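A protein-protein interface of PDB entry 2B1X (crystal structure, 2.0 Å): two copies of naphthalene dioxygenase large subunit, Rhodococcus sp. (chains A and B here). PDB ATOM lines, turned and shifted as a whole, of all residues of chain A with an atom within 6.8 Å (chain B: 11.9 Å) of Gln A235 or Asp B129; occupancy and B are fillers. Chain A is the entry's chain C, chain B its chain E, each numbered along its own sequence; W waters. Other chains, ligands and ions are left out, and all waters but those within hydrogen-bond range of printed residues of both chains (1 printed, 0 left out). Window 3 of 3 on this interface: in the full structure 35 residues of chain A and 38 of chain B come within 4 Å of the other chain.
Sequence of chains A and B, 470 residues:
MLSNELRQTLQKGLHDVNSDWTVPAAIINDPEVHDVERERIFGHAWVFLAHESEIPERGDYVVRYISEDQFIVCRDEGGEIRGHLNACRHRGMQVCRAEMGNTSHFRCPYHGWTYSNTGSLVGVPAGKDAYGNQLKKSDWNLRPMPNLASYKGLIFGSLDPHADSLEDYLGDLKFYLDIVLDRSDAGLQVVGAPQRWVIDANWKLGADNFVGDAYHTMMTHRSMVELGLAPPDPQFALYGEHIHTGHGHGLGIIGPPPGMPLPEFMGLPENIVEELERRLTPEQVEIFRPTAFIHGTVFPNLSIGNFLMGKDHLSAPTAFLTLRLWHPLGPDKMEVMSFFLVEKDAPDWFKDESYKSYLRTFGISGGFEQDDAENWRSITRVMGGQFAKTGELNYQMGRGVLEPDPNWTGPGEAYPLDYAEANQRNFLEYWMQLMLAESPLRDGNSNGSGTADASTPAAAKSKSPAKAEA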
ATOM      1  N   MET A 218      -7.978 -23.848 -20.402  1.00  0.00           N
ATOM      2  CA  MET A 218      -8.773 -24.407 -21.501  1.00  0.00           C
ATOM      3  C   MET A 218      -8.060 -24.402 -22.830  1.00  0.00           C
ATOM      4  O   MET A 218      -8.306 -25.261 -23.668  1.00  0.00           O
ATOM      5  CB  MET A 218     -10.136 -23.700 -21.667  1.00  0.00           C
ATOM      6  CG  MET A 218     -11.085 -23.787 -20.473  1.00  0.00           C
ATOM      7  SD  MET A 218     -12.624 -22.860 -20.902  1.00  0.00           S
ATOM      8  CE  MET A 218     -12.095 -21.183 -20.559  1.00  0.00           C
ATOM      9  N   PRO A 232     -11.984 -31.380 -17.694  1.00  0.00           N
ATOM     10  CA  PRO A 232     -12.676 -31.275 -18.992  1.00  0.00           C
ATOM     11  C   PRO A 232     -13.815 -30.249 -19.024  1.00  0.00           C
ATOM     12  O   PRO A 232     -14.212 -29.795 -20.106  1.00  0.00           O
ATOM     13  CB  PRO A 232     -13.235 -32.686 -19.209  1.00  0.00           C
ATOM     14  CG  PRO A 232     -13.443 -33.242 -17.827  1.00  0.00           C
ATOM     15  CD  PRO A 232     -12.398 -32.578 -16.942  1.00  0.00           C
ATOM     16  N   ASP A 233     -14.350 -29.906 -17.860  1.00  0.00           N
ATOM     17  CA  ASP A 233     -15.458 -28.952 -17.782  1.00  0.00           C
ATOM     18  C   ASP A 233     -14.946 -27.540 -18.032  1.00  0.00           C
ATOM     19  O   ASP A 233     -14.141 -27.030 -17.259  1.00  0.00           O
ATOM     20  CB  ASP A 233     -16.113 -29.024 -16.404  1.00  0.00           C
ATOM     21  CG  ASP A 233     -17.389 -28.205 -16.310  1.00  0.00           C
ATOM     22  OD1 ASP A 233     -17.790 -27.523 -17.294  1.00  0.00           O
ATOM     23  OD2 ASP A 233     -18.065 -28.196 -15.258  1.00  0.00           O
ATOM     24  N   PRO A 234     -15.424 -26.895 -19.096  1.00  0.00           N
ATOM     25  CA  PRO A 234     -15.023 -25.511 -19.379  1.00  0.00           C
ATOM     26  C   PRO A 234     -15.432 -24.546 -18.261  1.00  0.00           C
ATOM     27  O   PRO A 234     -14.889 -23.440 -18.187  1.00  0.00           O
ATOM     28  CB  PRO A 234     -15.746 -25.174 -20.690  1.00  0.00           C
ATOM     29  CG  PRO A 234     -16.518 -26.376 -21.096  1.00  0.00           C
ATOM     30  CD  PRO A 234     -16.385 -27.425 -20.084  1.00  0.00           C
ATOM     31  N   GLN A 235     -16.352 -24.963 -17.398  1.00  0.00           N
ATOM     32  CA  GLN A 235     -16.813 -24.132 -16.278  1.00  0.00           C
ATOM     33  C   GLN A 235     -16.119 -24.484 -14.970  1.00  0.00           C
ATOM     34  O   GLN A 235     -16.540 -24.043 -13.899  1.00  0.00           O
ATOM     35  CB  GLN A 235     -18.306 -24.339 -16.063  1.00  0.00           C
ATOM     36  CG  GLN A 235     -19.183 -23.928 -17.230  1.00  0.00           C
ATOM     37  CD  GLN A 235     -20.629 -23.920 -16.846  1.00  0.00           C
ATOM     38  OE1 GLN A 235     -21.112 -24.878 -16.211  1.00  0.00           O
ATOM     39  NE2 GLN A 235     -21.343 -22.838 -17.196  1.00  0.00           N
ATOM     40  N   PHE A 236     -15.073 -25.293 -15.040  1.00  0.00           N
ATOM     41  CA  PHE A 236     -14.488 -25.852 -13.819  1.00  0.00           C
ATOM     42  C   PHE A 236     -14.134 -24.802 -12.755  1.00  0.00           C
ATOM     43  O   PHE A 236     -14.232 -25.083 -11.551  1.00  0.00           O
ATOM     44  CB  PHE A 236     -13.282 -26.754 -14.136  1.00  0.00           C
ATOM     45  CG  PHE A 236     -11.988 -26.000 -14.366  1.00  0.00           C
ATOM     46  CD1 PHE A 236     -10.978 -26.029 -13.397  1.00  0.00           C
ATOM     47  CD2 PHE A 236     -11.781 -25.279 -15.546  1.00  0.00           C
ATOM     48  CE1 PHE A 236      -9.752 -25.352 -13.594  1.00  0.00           C
ATOM     49  CE2 PHE A 236     -10.576 -24.588 -15.756  1.00  0.00           C
ATOM     50  CZ  PHE A 236      -9.555 -24.629 -14.768  1.00  0.00           C
ATOM     51  N   ALA A 237     -13.709 -23.613 -13.189  1.00  0.00           N
ATOM     52  CA  ALA A 237     -13.172 -22.635 -12.230  1.00  0.00           C
ATOM     53  C   ALA A 237     -14.283 -21.780 -11.619  1.00  0.00           C
ATOM     54  O   ALA A 237     -14.018 -20.951 -10.743  1.00  0.00           O
ATOM     55  CB  ALA A 237     -12.073 -21.764 -12.867  1.00  0.00           C
ATOM     56  N   LEU A 238     -15.529 -22.007 -12.057  1.00  0.00           N
ATOM     57  CA  LEU A 238     -16.694 -21.386 -11.423  1.00  0.00           C
ATOM     58  C   LEU A 238     -16.911 -21.987 -10.034  1.00  0.00           C
ATOM     59  O   LEU A 238     -17.482 -21.340  -9.148  1.00  0.00           O
ATOM     60  CB  LEU A 238     -17.971 -21.525 -12.289  1.00  0.00           C
ATOM     61  CG  LEU A 238     -18.063 -20.838 -13.672  1.00  0.00           C
ATOM     62  CD1 LEU A 238     -19.438 -21.012 -14.297  1.00  0.00           C
ATOM     63  CD2 LEU A 238     -17.690 -19.341 -13.608  1.00  0.00           C
ATOM     64  N   TYR A 239     -16.436 -23.221  -9.841  1.00  0.00           N
ATOM     65  CA  TYR A 239     -16.500 -23.864  -8.524  1.00  0.00           C
ATOM     66  C   TYR A 239     -15.235 -23.546  -7.742  1.00  0.00           C
ATOM     67  O   TYR A 239     -14.421 -24.441  -7.410  1.00  0.00           O
ATOM     68  CB  TYR A 239     -16.716 -25.373  -8.657  1.00  0.00           C
ATOM     69  CG  TYR A 239     -17.842 -25.705  -9.610  1.00  0.00           C
ATOM     70  CD1 TYR A 239     -17.581 -25.933 -10.956  1.00  0.00           C
ATOM     71  CD2 TYR A 239     -19.179 -25.742  -9.175  1.00  0.00           C
ATOM     72  CE1 TYR A 239     -18.615 -26.216 -11.860  1.00  0.00           C
ATOM     73  CE2 TYR A 239     -20.224 -26.023 -10.085  1.00  0.00           C
ATOM     74  CZ  TYR A 239     -19.919 -26.252 -11.418  1.00  0.00           C
ATOM     75  OH  TYR A 239     -20.930 -26.546 -12.320  1.00  0.00           O
ATOM     76  N   MET A 397     -11.499  -8.978 -17.088  1.00  0.00           N
ATOM     77  CA  MET A 397     -12.367 -10.086 -16.728  1.00  0.00           C
ATOM     78  C   MET A 397     -13.076  -9.788 -15.403  1.00  0.00           C
ATOM     79  O   MET A 397     -12.428  -9.663 -14.375  1.00  0.00           O
ATOM     80  CB  MET A 397     -11.571 -11.363 -16.626  1.00  0.00           C
ATOM     81  CG  MET A 397     -12.422 -12.584 -16.348  1.00  0.00           C
ATOM     82  SD  MET A 397     -11.361 -14.036 -16.137  1.00  0.00           S
ATOM     83  CE  MET A 397     -10.841 -14.266 -17.789  1.00  0.00           C
ATOM     84  N   LEU A 417     -15.865 -17.101  -7.577  1.00  0.00           N
ATOM     85  CA  LEU A 417     -15.518 -17.872  -8.772  1.00  0.00           C
ATOM     86  C   LEU A 417     -14.031 -17.662  -8.970  1.00  0.00           C
ATOM     87  O   LEU A 417     -13.472 -16.742  -8.417  1.00  0.00           O
ATOM     88  CB  LEU A 417     -16.292 -17.415 -10.024  1.00  0.00           C
ATOM     89  CG  LEU A 417     -15.945 -16.073 -10.676  1.00  0.00           C
ATOM     90  CD1 LEU A 417     -16.584 -15.912 -12.053  1.00  0.00           C
ATOM     91  CD2 LEU A 417     -16.324 -14.889  -9.777  1.00  0.00           C
ATOM     92  N   TYR A 419     -12.707 -17.487 -12.259  1.00  0.00           N
ATOM     93  CA  TYR A 419     -12.480 -16.773 -13.536  1.00  0.00           C
ATOM     94  C   TYR A 419     -12.586 -15.285 -13.224  1.00  0.00           C
ATOM     95  O   TYR A 419     -13.701 -14.693 -13.170  1.00  0.00           O
ATOM     96  CB  TYR A 419     -13.495 -17.178 -14.614  1.00  0.00           C
ATOM     97  CG  TYR A 419     -13.273 -18.547 -15.242  1.00  0.00           C
ATOM     98  CD1 TYR A 419     -14.360 -19.286 -15.738  1.00  0.00           C
ATOM     99  CD2 TYR A 419     -11.991 -19.098 -15.357  1.00  0.00           C
ATOM    100  CE1 TYR A 419     -14.174 -20.547 -16.328  1.00  0.00           C
ATOM    101  CE2 TYR A 419     -11.784 -20.350 -15.936  1.00  0.00           C
ATOM    102  CZ  TYR A 419     -12.889 -21.079 -16.414  1.00  0.00           C
ATOM    103  OH  TYR A 419     -12.704 -22.325 -16.990  1.00  0.00           O
ATOM    104  N   TRP B 113      -8.379 -16.558 -27.268  1.00  0.00           N
ATOM    105  CA  TRP B 113      -9.063 -15.446 -27.965  1.00  0.00           C
ATOM    106  C   TRP B 113      -8.828 -15.694 -29.445  1.00  0.00           C
ATOM    107  O   TRP B 113      -7.744 -16.025 -29.850  1.00  0.00           O
ATOM    108  CB  TRP B 113      -8.519 -14.067 -27.575  1.00  0.00           C
ATOM    109  CG  TRP B 113      -8.999 -13.549 -26.225  1.00  0.00           C
ATOM    110  CD1 TRP B 113      -9.442 -14.292 -25.168  1.00  0.00           C
ATOM    111  CD2 TRP B 113      -8.996 -12.180 -25.781  1.00  0.00           C
ATOM    112  NE1 TRP B 113      -9.727 -13.469 -24.093  1.00  0.00           N
ATOM    113  CE2 TRP B 113      -9.477 -12.167 -24.446  1.00  0.00           C
ATOM    114  CE3 TRP B 113      -8.654 -10.957 -26.379  1.00  0.00           C
ATOM    115  CZ2 TRP B 113      -9.649 -10.978 -23.705  1.00  0.00           C
ATOM    116  CZ3 TRP B 113      -8.821  -9.773 -25.630  1.00  0.00           C
ATOM    117  CH2 TRP B 113      -9.291  -9.803 -24.300  1.00  0.00           C
ATOM    118  N   GLY B 123     -14.128 -14.314 -31.167  1.00  0.00           N
ATOM    119  CA  GLY B 123     -14.425 -15.311 -30.154  1.00  0.00           C
ATOM    120  C   GLY B 123     -13.575 -15.177 -28.909  1.00  0.00           C
ATOM    121  O   GLY B 123     -12.366 -15.041 -28.985  1.00  0.00           O
ATOM    122  N   VAL B 124     -14.226 -15.234 -27.765  1.00  0.00           N
ATOM    123  CA  VAL B 124     -13.552 -15.226 -26.473  1.00  0.00           C
ATOM    124  C   VAL B 124     -14.157 -16.404 -25.688  1.00  0.00           C
ATOM    125  O   VAL B 124     -15.368 -16.430 -25.462  1.00  0.00           O
ATOM    126  CB  VAL B 124     -13.798 -13.846 -25.771  1.00  0.00           C
ATOM    127  CG1 VAL B 124     -13.497 -13.888 -24.280  1.00  0.00           C
ATOM    128  CG2 VAL B 124     -12.955 -12.733 -26.489  1.00  0.00           C
ATOM    129  N   PRO B 125     -13.333 -17.381 -25.296  1.00  0.00           N
ATOM    130  CA  PRO B 125     -13.767 -18.451 -24.371  1.00  0.00           C
ATOM    131  C   PRO B 125     -14.286 -17.884 -23.044  1.00  0.00           C
ATOM    132  O   PRO B 125     -13.691 -16.926 -22.526  1.00  0.00           O
ATOM    133  CB  PRO B 125     -12.468 -19.256 -24.162  1.00  0.00           C
ATOM    134  CG  PRO B 125     -11.686 -18.998 -25.465  1.00  0.00           C
ATOM    135  CD  PRO B 125     -11.920 -17.546 -25.717  1.00  0.00           C
ATOM    136  N   ALA B 126     -15.379 -18.452 -22.516  1.00  0.00           N
ATOM    137  CA  ALA B 126     -15.996 -17.987 -21.247  1.00  0.00           C
ATOM    138  C   ALA B 126     -16.508 -16.531 -21.333  1.00  0.00           C
ATOM    139  O   ALA B 126     -16.569 -15.828 -20.340  1.00  0.00           O
ATOM    140  CB  ALA B 126     -15.037 -18.172 -20.063  1.00  0.00           C
ATOM    141  N   GLY B 127     -16.868 -16.109 -22.544  1.00  0.00           N
ATOM    142  CA  GLY B 127     -17.460 -14.797 -22.777  1.00  0.00           C
ATOM    143  C   GLY B 127     -18.523 -14.475 -21.738  1.00  0.00           C
ATOM    144  O   GLY B 127     -18.640 -13.353 -21.280  1.00  0.00           O
ATOM    145  N   LYS B 128     -19.290 -15.495 -21.377  1.00  0.00           N
ATOM    146  CA  LYS B 128     -20.382 -15.388 -20.405  1.00  0.00           C
ATOM    147  C   LYS B 128     -19.925 -15.676 -18.999  1.00  0.00           C
ATOM    148  O   LYS B 128     -20.108 -14.860 -18.108  1.00  0.00           O
ATOM    149  CB  LYS B 128     -21.492 -16.375 -20.772  1.00  0.00           C
ATOM    150  CG  LYS B 128     -20.988 -17.534 -21.681  1.00  0.00           C
ATOM    151  CD  LYS B 128     -19.729 -18.298 -21.101  1.00  0.00           C
ATOM    152  CE  LYS B 128     -19.160 -19.201 -22.124  1.00  0.00           C
ATOM    153  NZ  LYS B 128     -19.607 -18.734 -23.458  1.00  0.00           N
ATOM    154  N   ASP B 129     -19.339 -16.848 -18.794  1.00  0.00           N
ATOM    155  CA  ASP B 129     -18.965 -17.290 -17.433  1.00  0.00           C
ATOM    156  C   ASP B 129     -17.874 -16.455 -16.773  1.00  0.00           C
ATOM    157  O   ASP B 129     -17.839 -16.331 -15.542  1.00  0.00           O
ATOM    158  CB  ASP B 129     -18.503 -18.747 -17.462  1.00  0.00           C
ATOM    159  CG  ASP B 129     -19.619 -19.714 -17.835  1.00  0.00           C
ATOM    160  OD1 ASP B 129     -19.269 -20.827 -18.309  1.00  0.00           O
ATOM    161  OD2 ASP B 129     -20.853 -19.467 -17.699  1.00  0.00           O
ATOM    162  N   ALA B 130     -16.958 -15.915 -17.581  1.00  0.00           N
ATOM    163  CA  ALA B 130     -15.843 -15.141 -17.029  1.00  0.00           C
ATOM    164  C   ALA B 130     -16.070 -13.653 -17.177  1.00  0.00           C
ATOM    165  O   ALA B 130     -15.814 -12.898 -16.238  1.00  0.00           O
ATOM    166  CB  ALA B 130     -14.521 -15.549 -17.681  1.00  0.00           C
ATOM    167  N   TYR B 131     -16.568 -13.247 -18.343  1.00  0.00           N
ATOM    168  CA  TYR B 131     -16.727 -11.823 -18.648  1.00  0.00           C
ATOM    169  C   TYR B 131     -18.126 -11.264 -18.502  1.00  0.00           C
ATOM    170  O   TYR B 131     -18.313 -10.059 -18.631  1.00  0.00           O
ATOM    171  CB  TYR B 131     -16.193 -11.525 -20.052  1.00  0.00           C
ATOM    172  CG  TYR B 131     -14.700 -11.666 -20.180  1.00  0.00           C
ATOM    173  CD1 TYR B 131     -14.151 -12.891 -20.560  1.00  0.00           C
ATOM    174  CD2 TYR B 131     -13.827 -10.572 -19.967  1.00  0.00           C
ATOM    175  CE1 TYR B 131     -12.774 -13.062 -20.723  1.00  0.00           C
ATOM    176  CE2 TYR B 131     -12.434 -10.736 -20.115  1.00  0.00           C
ATOM    177  CZ  TYR B 131     -11.927 -11.998 -20.515  1.00  0.00           C
ATOM    178  OH  TYR B 131     -10.598 -12.271 -20.699  1.00  0.00           O
ATOM    179  N   GLY B 132     -19.100 -12.135 -18.240  1.00  0.00           N
ATOM    180  CA  GLY B 132     -20.500 -11.735 -18.076  1.00  0.00           C
ATOM    181  C   GLY B 132     -21.020 -10.967 -19.272  1.00  0.00           C
ATOM    182  O   GLY B 132     -21.829 -10.063 -19.112  1.00  0.00           O
ATOM    183  N   ASN B 133     -20.502 -11.305 -20.463  1.00  0.00           N
ATOM    184  CA  ASN B 133     -20.807 -10.611 -21.716  1.00  0.00           C
ATOM    185  C   ASN B 133     -20.565  -9.092 -21.678  1.00  0.00           C
ATOM    186  O   ASN B 133     -21.195  -8.353 -22.432  1.00  0.00           O
ATOM    187  CB  ASN B 133     -22.265 -10.887 -22.171  1.00  0.00           C
ATOM    188  CG  ASN B 133     -22.480 -12.328 -22.645  1.00  0.00           C
ATOM    189  OD1 ASN B 133     -23.441 -13.013 -22.254  1.00  0.00           O
ATOM    190  ND2 ASN B 133     -21.579 -12.794 -23.477  1.00  0.00           N
ATOM    191  N   GLN B 134     -19.653  -8.640 -20.816  1.00  0.00           N
ATOM    192  CA  GLN B 134     -19.316  -7.220 -20.729  1.00  0.00           C
ATOM    193  C   GLN B 134     -18.108  -6.810 -21.562  1.00  0.00           C
ATOM    194  O   GLN B 134     -17.836  -5.623 -21.717  1.00  0.00           O
ATOM    195  CB  GLN B 134     -19.064  -6.801 -19.269  1.00  0.00           C
ATOM    196  CG  GLN B 134     -20.171  -7.128 -18.324  1.00  0.00           C
ATOM    197  CD  GLN B 134     -21.434  -6.384 -18.647  1.00  0.00           C
ATOM    198  OE1 GLN B 134     -21.474  -5.150 -18.570  1.00  0.00           O
ATOM    199  NE2 GLN B 134     -22.452  -7.122 -19.070  1.00  0.00           N
ATOM    200  N   LEU B 135     -17.362  -7.776 -22.074  1.00  0.00           N
ATOM    201  CA  LEU B 135     -16.215  -7.441 -22.917  1.00  0.00           C
ATOM    202  C   LEU B 135     -16.664  -7.076 -24.328  1.00  0.00           C
ATOM    203  O   LEU B 135     -17.248  -7.912 -25.018  1.00  0.00           O
ATOM    204  CB  LEU B 135     -15.205  -8.582 -22.963  1.00  0.00           C
ATOM    205  CG  LEU B 135     -13.938  -8.306 -23.796  1.00  0.00           C
ATOM    206  CD1 LEU B 135     -12.896  -7.517 -22.995  1.00  0.00           C
ATOM    207  CD2 LEU B 135     -13.345  -9.623 -24.273  1.00  0.00           C
ATOM    208  N   LYS B 137     -15.887  -6.850 -27.711  1.00  0.00           N
ATOM    209  CA  LYS B 137     -14.902  -7.451 -28.630  1.00  0.00           C
ATOM    210  C   LYS B 137     -14.331  -6.517 -29.707  1.00  0.00           C
ATOM    211  O   LYS B 137     -13.119  -6.578 -30.026  1.00  0.00           O
ATOM    212  CB  LYS B 137     -15.482  -8.718 -29.271  1.00  0.00           C
ATOM    213  CG  LYS B 137     -15.615  -9.882 -28.253  1.00  0.00           C
ATOM    214  CD  LYS B 137     -15.694 -11.304 -28.901  1.00  0.00           C
ATOM    215  CE  LYS B 137     -16.930 -11.488 -29.823  1.00  0.00           C
ATOM    216  NZ  LYS B 137     -18.208 -11.255 -29.094  1.00  0.00           N
HETATM  217  O   HOH W   1     -15.340 -12.596 -13.715  1.00  0.00           O
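No position is printed for both chains.
Of the 6 pairs that touch across the chains among the printed residues, none has its exchanged pair printed and touching as well.
The side-chain carboxylate (OD1) of Asp B129 sits at hydrogen-bond distance from the side-chain amide nitrogen (NE2) of Gln A235.
O of Ala B126 sits at hydrogen-bond distance from N of Tyr B131 (3.3 Å).
OD1 of Asp A233 sits at hydrogen-bond distance from N of Gln A235 (2.9 Å).
O of Pro A234 lies within hydrogen-bond range of OH of Tyr A419 (2.7 Å).
Water W1 lies within hydrogen-bond range of the backbone carbonyl oxygen (O) of Ala B130 (2.6 Å) and the backbone carbonyl oxygen (O) of Tyr A419 (2.7 Å).
Leu A238 touches Asp B129.
Ala B130 touches Met A397.
Met A397 touches Tyr B131.
Leu A417 touches Asp B129.
Tyr A419 touches Ala B130.
Of the 12 printed residues of chain A, 5 touch a printed residue of chain B.
Printed residues of chain A that touch a printed residue of chain B: Gln A235, Leu A238, Met A397, Leu A417 and Tyr A419.
Hydrophobic or aromatic side chains of chain A within 4 Å of the printed part of chain B: Leu A238, Met A397, Leu A417 and Tyr A419.
Among the printed residues, 6 pairs touch across the chains.
No residue of chain B comes within 4 Å of Asp A233.
Gln A235 touches just one residue of chain B: Asp B129 (3.1 Å).
No residue of chain B comes within 4 Å of Phe A236.
No residue of chain B comes within 4 Å of Ala A237.
Of chain B, only Asp B129 comes within 4 Å of Leu A238.
No residue of chain B comes within 4 Å of Tyr A239.
Of the printed residues of chain B, Met A397 touches Ala B130 (3.4 Å) and Tyr B131 (3.4 Å).
Of the printed residues of chain B, Leu A417 touches Asp B129.
Printed residues of chain A within 4 Å of Ala B130: Met A397 (3.4 Å) and Tyr A419 (3.6 Å).
Of the printed residues of chain A, Tyr B131 touches Met A397 (3.4 Å).
Gly B132 touches none of the printed residues of chain A.
Gln B134 touches none of the printed residues of chain A.
The nearest residue of chain B that does not touch Gln A235 is Lys B128 (6.2 Å).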
